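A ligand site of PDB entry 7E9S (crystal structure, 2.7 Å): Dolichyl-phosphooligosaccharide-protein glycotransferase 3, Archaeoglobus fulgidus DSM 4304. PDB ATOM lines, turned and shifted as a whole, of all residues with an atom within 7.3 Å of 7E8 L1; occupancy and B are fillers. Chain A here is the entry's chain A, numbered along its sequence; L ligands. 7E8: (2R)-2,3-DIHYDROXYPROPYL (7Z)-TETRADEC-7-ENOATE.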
ATOM      1  N   TRP A  33      -3.168  -4.676 -24.214  1.00  0.00           N
ATOM      2  CA  TRP A  33      -1.967  -4.122 -23.581  1.00  0.00           C
ATOM      3  C   TRP A  33      -0.944  -3.700 -24.617  1.00  0.00           C
ATOM      4  O   TRP A  33      -0.368  -2.599 -24.525  1.00  0.00           O
ATOM      5  CB  TRP A  33      -1.363  -5.140 -22.617  1.00  0.00           C
ATOM      6  CG  TRP A  33      -0.202  -4.592 -21.843  1.00  0.00           C
ATOM      7  CD1 TRP A  33       1.092  -4.514 -22.259  1.00  0.00           C
ATOM      8  CD2 TRP A  33      -0.232  -4.024 -20.524  1.00  0.00           C
ATOM      9  NE1 TRP A  33       1.870  -3.939 -21.284  1.00  0.00           N
ATOM     10  CE2 TRP A  33       1.087  -3.629 -20.212  1.00  0.00           C
ATOM     11  CE3 TRP A  33      -1.243  -3.816 -19.584  1.00  0.00           C
ATOM     12  CZ2 TRP A  33       1.412  -3.039 -18.995  1.00  0.00           C
ATOM     13  CZ3 TRP A  33      -0.913  -3.230 -18.380  1.00  0.00           C
ATOM     14  CH2 TRP A  33       0.403  -2.847 -18.088  1.00  0.00           C
ATOM     15  N   VAL A  36      -1.978  -0.358 -26.453  1.00  0.00           N
ATOM     16  CA  VAL A  36      -1.916   0.900 -25.718  1.00  0.00           C
ATOM     17  C   VAL A  36      -0.485   1.288 -25.379  1.00  0.00           C
ATOM     18  O   VAL A  36      -0.104   2.454 -25.504  1.00  0.00           O
ATOM     19  CB  VAL A  36      -2.783   0.804 -24.449  1.00  0.00           C
ATOM     20  CG1 VAL A  36      -2.733   2.098 -23.652  1.00  0.00           C
ATOM     21  CG2 VAL A  36      -4.221   0.466 -24.819  1.00  0.00           C
ATOM     22  N   PHE A  37       0.346   0.324 -24.970  1.00  0.00           N
ATOM     23  CA  PHE A  37       1.721   0.599 -24.569  1.00  0.00           C
ATOM     24  C   PHE A  37       2.652   0.184 -25.708  1.00  0.00           C
ATOM     25  O   PHE A  37       3.128  -0.952 -25.768  1.00  0.00           O
ATOM     26  CB  PHE A  37       2.049  -0.124 -23.259  1.00  0.00           C
ATOM     27  CG  PHE A  37       1.271   0.394 -22.086  1.00  0.00           C
ATOM     28  CD1 PHE A  37       1.525   1.656 -21.567  1.00  0.00           C
ATOM     29  CD2 PHE A  37       0.262  -0.370 -21.507  1.00  0.00           C
ATOM     30  CE1 PHE A  37       0.802   2.137 -20.495  1.00  0.00           C
ATOM     31  CE2 PHE A  37      -0.457   0.105 -20.424  1.00  0.00           C
ATOM     32  CZ  PHE A  37      -0.185   1.365 -19.919  1.00  0.00           C
ATOM     33  N   THR A  38       2.920   1.125 -26.619  1.00  0.00           N
ATOM     34  CA  THR A  38       3.812   0.909 -27.754  1.00  0.00           C
ATOM     35  C   THR A  38       4.928   1.938 -27.762  1.00  0.00           C
ATOM     36  O   THR A  38       5.444   2.339 -26.708  1.00  0.00           O
ATOM     37  CB  THR A  38       3.043   0.980 -29.079  1.00  0.00           C
ATOM     38  OG1 THR A  38       2.177   2.127 -29.077  1.00  0.00           O
ATOM     39  CG2 THR A  38       2.231  -0.265 -29.305  1.00  0.00           C
ATOM     40  N   TRP A  39       5.338   2.360 -28.964  1.00  0.00           N
ATOM     41  CA  TRP A  39       6.135   3.574 -29.165  1.00  0.00           C
ATOM     42  C   TRP A  39       5.670   4.783 -28.360  1.00  0.00           C
ATOM     43  O   TRP A  39       6.494   5.658 -28.065  1.00  0.00           O
ATOM     44  CB  TRP A  39       6.220   3.859 -30.682  1.00  0.00           C
ATOM     45  CG  TRP A  39       4.913   3.669 -31.447  1.00  0.00           C
ATOM     46  CD1 TRP A  39       4.520   2.520 -32.072  1.00  0.00           C
ATOM     47  CD2 TRP A  39       3.841   4.605 -31.622  1.00  0.00           C
ATOM     48  NE1 TRP A  39       3.291   2.693 -32.660  1.00  0.00           N
ATOM     49  CE2 TRP A  39       2.842   3.963 -32.395  1.00  0.00           C
ATOM     50  CE3 TRP A  39       3.621   5.929 -31.224  1.00  0.00           C
ATOM     51  CZ2 TRP A  39       1.651   4.585 -32.760  1.00  0.00           C
ATOM     52  CZ3 TRP A  39       2.443   6.554 -31.591  1.00  0.00           C
ATOM     53  CH2 TRP A  39       1.468   5.875 -32.357  1.00  0.00           C
ATOM     54  N   THR A  40       4.389   4.874 -27.989  1.00  0.00           N
ATOM     55  CA  THR A  40       3.974   5.801 -26.953  1.00  0.00           C
ATOM     56  C   THR A  40       2.779   5.196 -26.237  1.00  0.00           C
ATOM     57  O   THR A  40       2.282   4.135 -26.622  1.00  0.00           O
ATOM     58  CB  THR A  40       3.646   7.192 -27.520  1.00  0.00           C
ATOM     59  OG1 THR A  40       3.659   8.158 -26.454  1.00  0.00           O
ATOM     60  CG2 THR A  40       2.280   7.212 -28.172  1.00  0.00           C
ATOM     61  N   VAL A  41       2.319   5.853 -25.180  1.00  0.00           N
ATOM     62  CA  VAL A  41       1.084   5.437 -24.531  1.00  0.00           C
ATOM     63  C   VAL A  41      -0.062   6.013 -25.358  1.00  0.00           C
ATOM     64  O   VAL A  41      -0.239   7.235 -25.441  1.00  0.00           O
ATOM     65  CB  VAL A  41       1.003   5.896 -23.069  1.00  0.00           C
ATOM     66  CG1 VAL A  41      -0.385   5.618 -22.508  1.00  0.00           C
ATOM     67  CG2 VAL A  41       2.048   5.187 -22.234  1.00  0.00           C
ATOM     68  N   ARG A  42      -0.835   5.135 -25.999  1.00  0.00           N
ATOM     69  CA  ARG A  42      -1.901   5.539 -26.919  1.00  0.00           C
ATOM     70  C   ARG A  42      -3.228   5.499 -26.180  1.00  0.00           C
ATOM     71  O   ARG A  42      -3.778   4.420 -25.934  1.00  0.00           O
ATOM     72  CB  ARG A  42      -1.933   4.632 -28.146  1.00  0.00           C
ATOM     73  CG  ARG A  42      -0.846   4.886 -29.155  1.00  0.00           C
ATOM     74  CD  ARG A  42      -0.886   3.842 -30.266  1.00  0.00           C
ATOM     75  NE  ARG A  42      -2.021   4.020 -31.168  1.00  0.00           N
ATOM     76  CZ  ARG A  42      -2.971   3.122 -31.362  1.00  0.00           C
ATOM     77  NH1 ARG A  42      -2.940   1.971 -30.698  1.00  0.00           N
ATOM     78  NH2 ARG A  42      -3.953   3.365 -32.223  1.00  0.00           N
ATOM     79  N   LEU A  89     -11.288  12.714 -11.083  1.00  0.00           N
ATOM     80  CA  LEU A  89     -10.779  11.375 -10.803  1.00  0.00           C
ATOM     81  C   LEU A  89      -9.382  11.188 -11.373  1.00  0.00           C
ATOM     82  O   LEU A  89      -8.444  10.815 -10.659  1.00  0.00           O
ATOM     83  CB  LEU A  89     -11.733  10.325 -11.364  1.00  0.00           C
ATOM     84  CG  LEU A  89     -11.363   8.878 -11.060  1.00  0.00           C
ATOM     85  CD1 LEU A  89     -11.486   8.597  -9.577  1.00  0.00           C
ATOM     86  CD2 LEU A  89     -12.214   7.915 -11.873  1.00  0.00           C
ATOM     87  N   GLY A  90      -9.215  11.460 -12.677  1.00  0.00           N
ATOM     88  CA  GLY A  90      -7.906  11.346 -13.289  1.00  0.00           C
ATOM     89  C   GLY A  90      -6.898  12.312 -12.713  1.00  0.00           C
ATOM     90  O   GLY A  90      -5.717  11.987 -12.585  1.00  0.00           O
ATOM     91  N   ALA A  93      -5.868  10.848  -9.401  1.00  0.00           N
ATOM     92  CA  ALA A  93      -5.096   9.639  -9.690  1.00  0.00           C
ATOM     93  C   ALA A  93      -3.699   9.980 -10.173  1.00  0.00           C
ATOM     94  O   ALA A  93      -2.728   9.283  -9.858  1.00  0.00           O
ATOM     95  CB  ALA A  93      -5.830   8.776 -10.713  1.00  0.00           C
ATOM     96  N   GLY A  94      -3.562  11.052 -10.954  1.00  0.00           N
ATOM     97  CA  GLY A  94      -2.247  11.444 -11.436  1.00  0.00           C
ATOM     98  C   GLY A  94      -1.355  11.959 -10.330  1.00  0.00           C
ATOM     99  O   GLY A  94      -0.141  11.708 -10.324  1.00  0.00           O
ATOM    100  N   PHE A  97       0.003   9.039  -8.080  1.00  0.00           N
ATOM    101  CA  PHE A  97       1.095   8.343  -8.736  1.00  0.00           C
ATOM    102  C   PHE A  97       2.158   9.291  -9.275  1.00  0.00           C
ATOM    103  O   PHE A  97       3.011   8.865 -10.067  1.00  0.00           O
ATOM    104  CB  PHE A  97       0.543   7.467  -9.873  1.00  0.00           C
ATOM    105  CG  PHE A  97      -0.275   6.301  -9.388  1.00  0.00           C
ATOM    106  CD1 PHE A  97       0.330   5.090  -9.109  1.00  0.00           C
ATOM    107  CD2 PHE A  97      -1.641   6.431  -9.191  1.00  0.00           C
ATOM    108  CE1 PHE A  97      -0.421   4.017  -8.648  1.00  0.00           C
ATOM    109  CE2 PHE A  97      -2.393   5.367  -8.727  1.00  0.00           C
ATOM    110  CZ  PHE A  97      -1.791   4.153  -8.464  1.00  0.00           C
ATOM    111  N   GLU A 103       3.583  11.402 -21.086  1.00  0.00           N
ATOM    112  CA  GLU A 103       3.327   9.979 -21.266  1.00  0.00           C
ATOM    113  C   GLU A 103       3.049   9.280 -19.947  1.00  0.00           C
ATOM    114  O   GLU A 103       2.243   8.346 -19.901  1.00  0.00           O
ATOM    115  CB  GLU A 103       4.533   9.333 -21.966  1.00  0.00           C
ATOM    116  CG  GLU A 103       4.391   7.851 -22.261  1.00  0.00           C
ATOM    117  CD  GLU A 103       5.486   7.351 -23.173  1.00  0.00           C
ATOM    118  OE1 GLU A 103       5.809   6.142 -23.123  1.00  0.00           O
ATOM    119  OE2 GLU A 103       6.022   8.158 -23.949  1.00  0.00           O
ATOM    120  N   SER A 104       3.684   9.725 -18.859  1.00  0.00           N
ATOM    121  CA  SER A 104       3.465   9.085 -17.563  1.00  0.00           C
ATOM    122  C   SER A 104       2.053   9.315 -17.057  1.00  0.00           C
ATOM    123  O   SER A 104       1.496   8.454 -16.376  1.00  0.00           O
ATOM    124  CB  SER A 104       4.492   9.594 -16.545  1.00  0.00           C
ATOM    125  OG  SER A 104       4.177  10.912 -16.119  1.00  0.00           O
ATOM    126  N   ALA A 107      -0.325   6.892 -18.957  1.00  0.00           N
ATOM    127  CA  ALA A 107      -0.257   5.522 -18.478  1.00  0.00           C
ATOM    128  C   ALA A 107      -1.172   5.311 -17.274  1.00  0.00           C
ATOM    129  O   ALA A 107      -1.758   4.230 -17.116  1.00  0.00           O
ATOM    130  CB  ALA A 107       1.177   5.152 -18.125  1.00  0.00           C
ATOM    131  N   VAL A 108      -1.313   6.322 -16.424  1.00  0.00           N
ATOM    132  CA  VAL A 108      -2.240   6.204 -15.293  1.00  0.00           C
ATOM    133  C   VAL A 108      -3.679   6.291 -15.774  1.00  0.00           C
ATOM    134  O   VAL A 108      -4.531   5.494 -15.360  1.00  0.00           O
ATOM    135  CB  VAL A 108      -1.924   7.287 -14.234  1.00  0.00           C
ATOM    136  CG1 VAL A 108      -2.966   7.256 -13.131  1.00  0.00           C
ATOM    137  CG2 VAL A 108      -0.527   7.089 -13.671  1.00  0.00           C
ATOM    138  N   LEU A 109      -3.968   7.242 -16.666  1.00  0.00           N
ATOM    139  CA  LEU A 109      -5.341   7.421 -17.147  1.00  0.00           C
ATOM    140  C   LEU A 109      -5.845   6.235 -17.952  1.00  0.00           C
ATOM    141  O   LEU A 109      -7.060   6.030 -18.033  1.00  0.00           O
ATOM    142  CB  LEU A 109      -5.442   8.690 -17.985  1.00  0.00           C
ATOM    143  CG  LEU A 109      -4.994   9.996 -17.334  1.00  0.00           C
ATOM    144  CD1 LEU A 109      -5.139  11.163 -18.306  1.00  0.00           C
ATOM    145  CD2 LEU A 109      -5.765  10.260 -16.058  1.00  0.00           C
ATOM    146  N   ALA A 110      -4.937   5.447 -18.553  1.00  0.00           N
ATOM    147  CA  ALA A 110      -5.369   4.330 -19.379  1.00  0.00           C
ATOM    148  C   ALA A 110      -6.077   3.248 -18.560  1.00  0.00           C
ATOM    149  O   ALA A 110      -6.917   2.517 -19.100  1.00  0.00           O
ATOM    150  CB  ALA A 110      -4.170   3.725 -20.114  1.00  0.00           C
ATOM    151  N   PHE A 111      -5.758   3.129 -17.271  1.00  0.00           N
ATOM    152  CA  PHE A 111      -6.355   2.093 -16.449  1.00  0.00           C
ATOM    153  C   PHE A 111      -7.735   2.471 -15.922  1.00  0.00           C
ATOM    154  O   PHE A 111      -8.518   1.576 -15.594  1.00  0.00           O
ATOM    155  CB  PHE A 111      -5.439   1.766 -15.271  1.00  0.00           C
ATOM    156  CG  PHE A 111      -4.221   0.973 -15.655  1.00  0.00           C
ATOM    157  CD1 PHE A 111      -4.298  -0.390 -15.871  1.00  0.00           C
ATOM    158  CD2 PHE A 111      -3.004   1.606 -15.823  1.00  0.00           C
ATOM    159  CE1 PHE A 111      -3.176  -1.116 -16.240  1.00  0.00           C
ATOM    160  CE2 PHE A 111      -1.878   0.893 -16.196  1.00  0.00           C
ATOM    161  CZ  PHE A 111      -1.964  -0.469 -16.392  1.00  0.00           C
ATOM    162  N   ILE A 112      -8.049   3.772 -15.841  1.00  0.00           N
ATOM    163  CA  ILE A 112      -9.328   4.198 -15.290  1.00  0.00           C
ATOM    164  C   ILE A 112     -10.516   3.600 -16.055  1.00  0.00           C
ATOM    165  O   ILE A 112     -11.421   3.064 -15.406  1.00  0.00           O
ATOM    166  CB  ILE A 112      -9.390   5.731 -15.225  1.00  0.00           C
ATOM    167  CG1 ILE A 112      -8.305   6.262 -14.288  1.00  0.00           C
ATOM    168  CG2 ILE A 112     -10.767   6.196 -14.780  1.00  0.00           C
ATOM    169  CD1 ILE A 112      -8.263   7.771 -14.211  1.00  0.00           C
ATOM    170  N   ILE A 115     -10.780  -0.157 -15.138  1.00  0.00           N
ATOM    171  CA  ILE A 115     -11.242  -0.392 -13.779  1.00  0.00           C
ATOM    172  C   ILE A 115     -12.736  -0.138 -13.662  1.00  0.00           C
ATOM    173  O   ILE A 115     -13.461  -0.873 -12.980  1.00  0.00           O
ATOM    174  CB  ILE A 115     -10.444   0.480 -12.789  1.00  0.00           C
ATOM    175  CG1 ILE A 115      -8.982   0.022 -12.750  1.00  0.00           C
ATOM    176  CG2 ILE A 115     -11.068   0.432 -11.393  1.00  0.00           C
ATOM    177  CD1 ILE A 115      -8.013   1.066 -12.222  1.00  0.00           C
HETATM  178  O22 7E8 L   1       5.342   2.807 -23.752  1.00  0.00           O
HETATM  179  C19 7E8 L   1       5.816   1.716 -22.922  1.00  0.00           C
HETATM  180  O20 7E8 L   1       5.890   3.549 -21.305  1.00  0.00           O
HETATM  181  C17 7E8 L   1       6.554   1.368 -20.495  1.00  0.00           C
HETATM  182  O16 7E8 L   1       5.387   1.685 -19.673  1.00  0.00           O
HETATM  183  C8  7E8 L   1       4.600   0.555 -19.279  1.00  0.00           C
HETATM  184  O15 7E8 L   1       5.045  -0.570 -19.520  1.00  0.00           O
HETATM  185  C7  7E8 L   1       3.235   0.797 -18.569  1.00  0.00           C
HETATM  186  C6  7E8 L   1       3.069   0.109 -17.174  1.00  0.00           C
HETATM  187  C5  7E8 L   1       1.810   0.589 -16.349  1.00  0.00           C
HETATM  188  C4  7E8 L   1       2.082   1.774 -15.341  1.00  0.00           C
HETATM  189  C3  7E8 L   1       0.825   2.349 -14.593  1.00  0.00           C
HETATM  190  C2  7E8 L   1       0.741   1.926 -13.136  1.00  0.00           C
HETATM  191  C1  7E8 L   1      -0.284   2.280 -12.309  1.00  0.00           C
HETATM  192  C9  7E8 L   1      -1.455   3.141 -12.767  1.00  0.00           C
HETATM  193  C10 7E8 L   1      -2.849   2.664 -12.212  1.00  0.00           C
HETATM  194  C11 7E8 L   1      -3.737   3.811 -11.589  1.00  0.00           C
HETATM  195  C12 7E8 L   1      -5.284   3.575 -11.661  1.00  0.00           C
HETATM  196  C13 7E8 L   1      -6.141   4.721 -11.032  1.00  0.00           C
HETATM  197  C14 7E8 L   1      -7.337   4.226 -10.156  1.00  0.00           C
HETATM  198  C18 7E8 L   1       6.593   2.347 -21.724  1.00  0.00           C
HETATM  199  O22 7E8 L   2     -13.881   5.092  -8.374  1.00  0.00           O
HETATM  200  C19 7E8 L   2     -13.833   5.550  -6.986  1.00  0.00           C
HETATM  201  O20 7E8 L   2     -15.388   5.463  -5.108  1.00  0.00           O
HETATM  202  C17 7E8 L   2     -15.700   7.304  -6.655  1.00  0.00           C
HETATM  203  O16 7E8 L   2     -15.302   8.021  -5.440  1.00  0.00           O
HETATM  204  C8  7E8 L   2     -14.363   9.077  -5.650  1.00  0.00           C
HETATM  205  O15 7E8 L   2     -13.161   8.817  -5.513  1.00  0.00           O
HETATM  206  C7  7E8 L   2     -14.867  10.495  -6.040  1.00  0.00           C
HETATM  207  C6  7E8 L   2     -13.783  11.368  -6.786  1.00  0.00           C
HETATM  208  C5  7E8 L   2     -14.004  12.923  -6.668  1.00  0.00           C
HETATM  209  C4  7E8 L   2     -14.722  13.585  -7.892  1.00  0.00           C
HETATM  210  C3  7E8 L   2     -16.054  14.347  -7.545  1.00  0.00           C
HETATM  211  C2  7E8 L   2     -15.918  15.862  -7.560  1.00  0.00           C
HETATM  212  C1  7E8 L   2     -16.585  16.686  -6.698  1.00  0.00           C
HETATM  213  C9  7E8 L   2     -17.546  16.159  -5.626  1.00  0.00           C
HETATM  214  C10 7E8 L   2     -17.986  17.259  -4.579  1.00  0.00           C
HETATM  215  C11 7E8 L   2     -19.473  17.157  -4.090  1.00  0.00           C
HETATM  216  C12 7E8 L   2     -19.854  18.168  -2.950  1.00  0.00           C
HETATM  217  C13 7E8 L   2     -21.361  18.143  -2.523  1.00  0.00           C
HETATM  218  C14 7E8 L   2     -21.655  18.819  -1.156  1.00  0.00           C
HETATM  219  C18 7E8 L   2     -15.306   5.784  -6.517  1.00  0.00           C
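The side-chain carboxylate of Glu 103 lies within hydrogen-bond range of an oxygen (O20) of 7E8 L1 (3.2 Å). O22 of 7E8 L1 lies within hydrogen-bond range of O of Thr 38.
The side-chain hydroxyl (OG1) of Thr 40 lies within hydrogen-bond range of the side-chain carboxylate (OE2) of Glu 103. The side-chain hydroxyl of Thr 38 sits at hydrogen-bond distance from the backbone carbonyl oxygen of Thr 40, at 3.2 Å.
Residues that only touch 7E8 L1: Phe 37 (3.4 Å), Phe 111 (3.5 Å), Phe 97 (3.5 Å), Ile 115 (3.7 Å), Val 108 (3.9 Å) and Trp 33 (3.996 Å). Of the 22 residues printed, 8 come within 4 Å of 7E8 L1.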
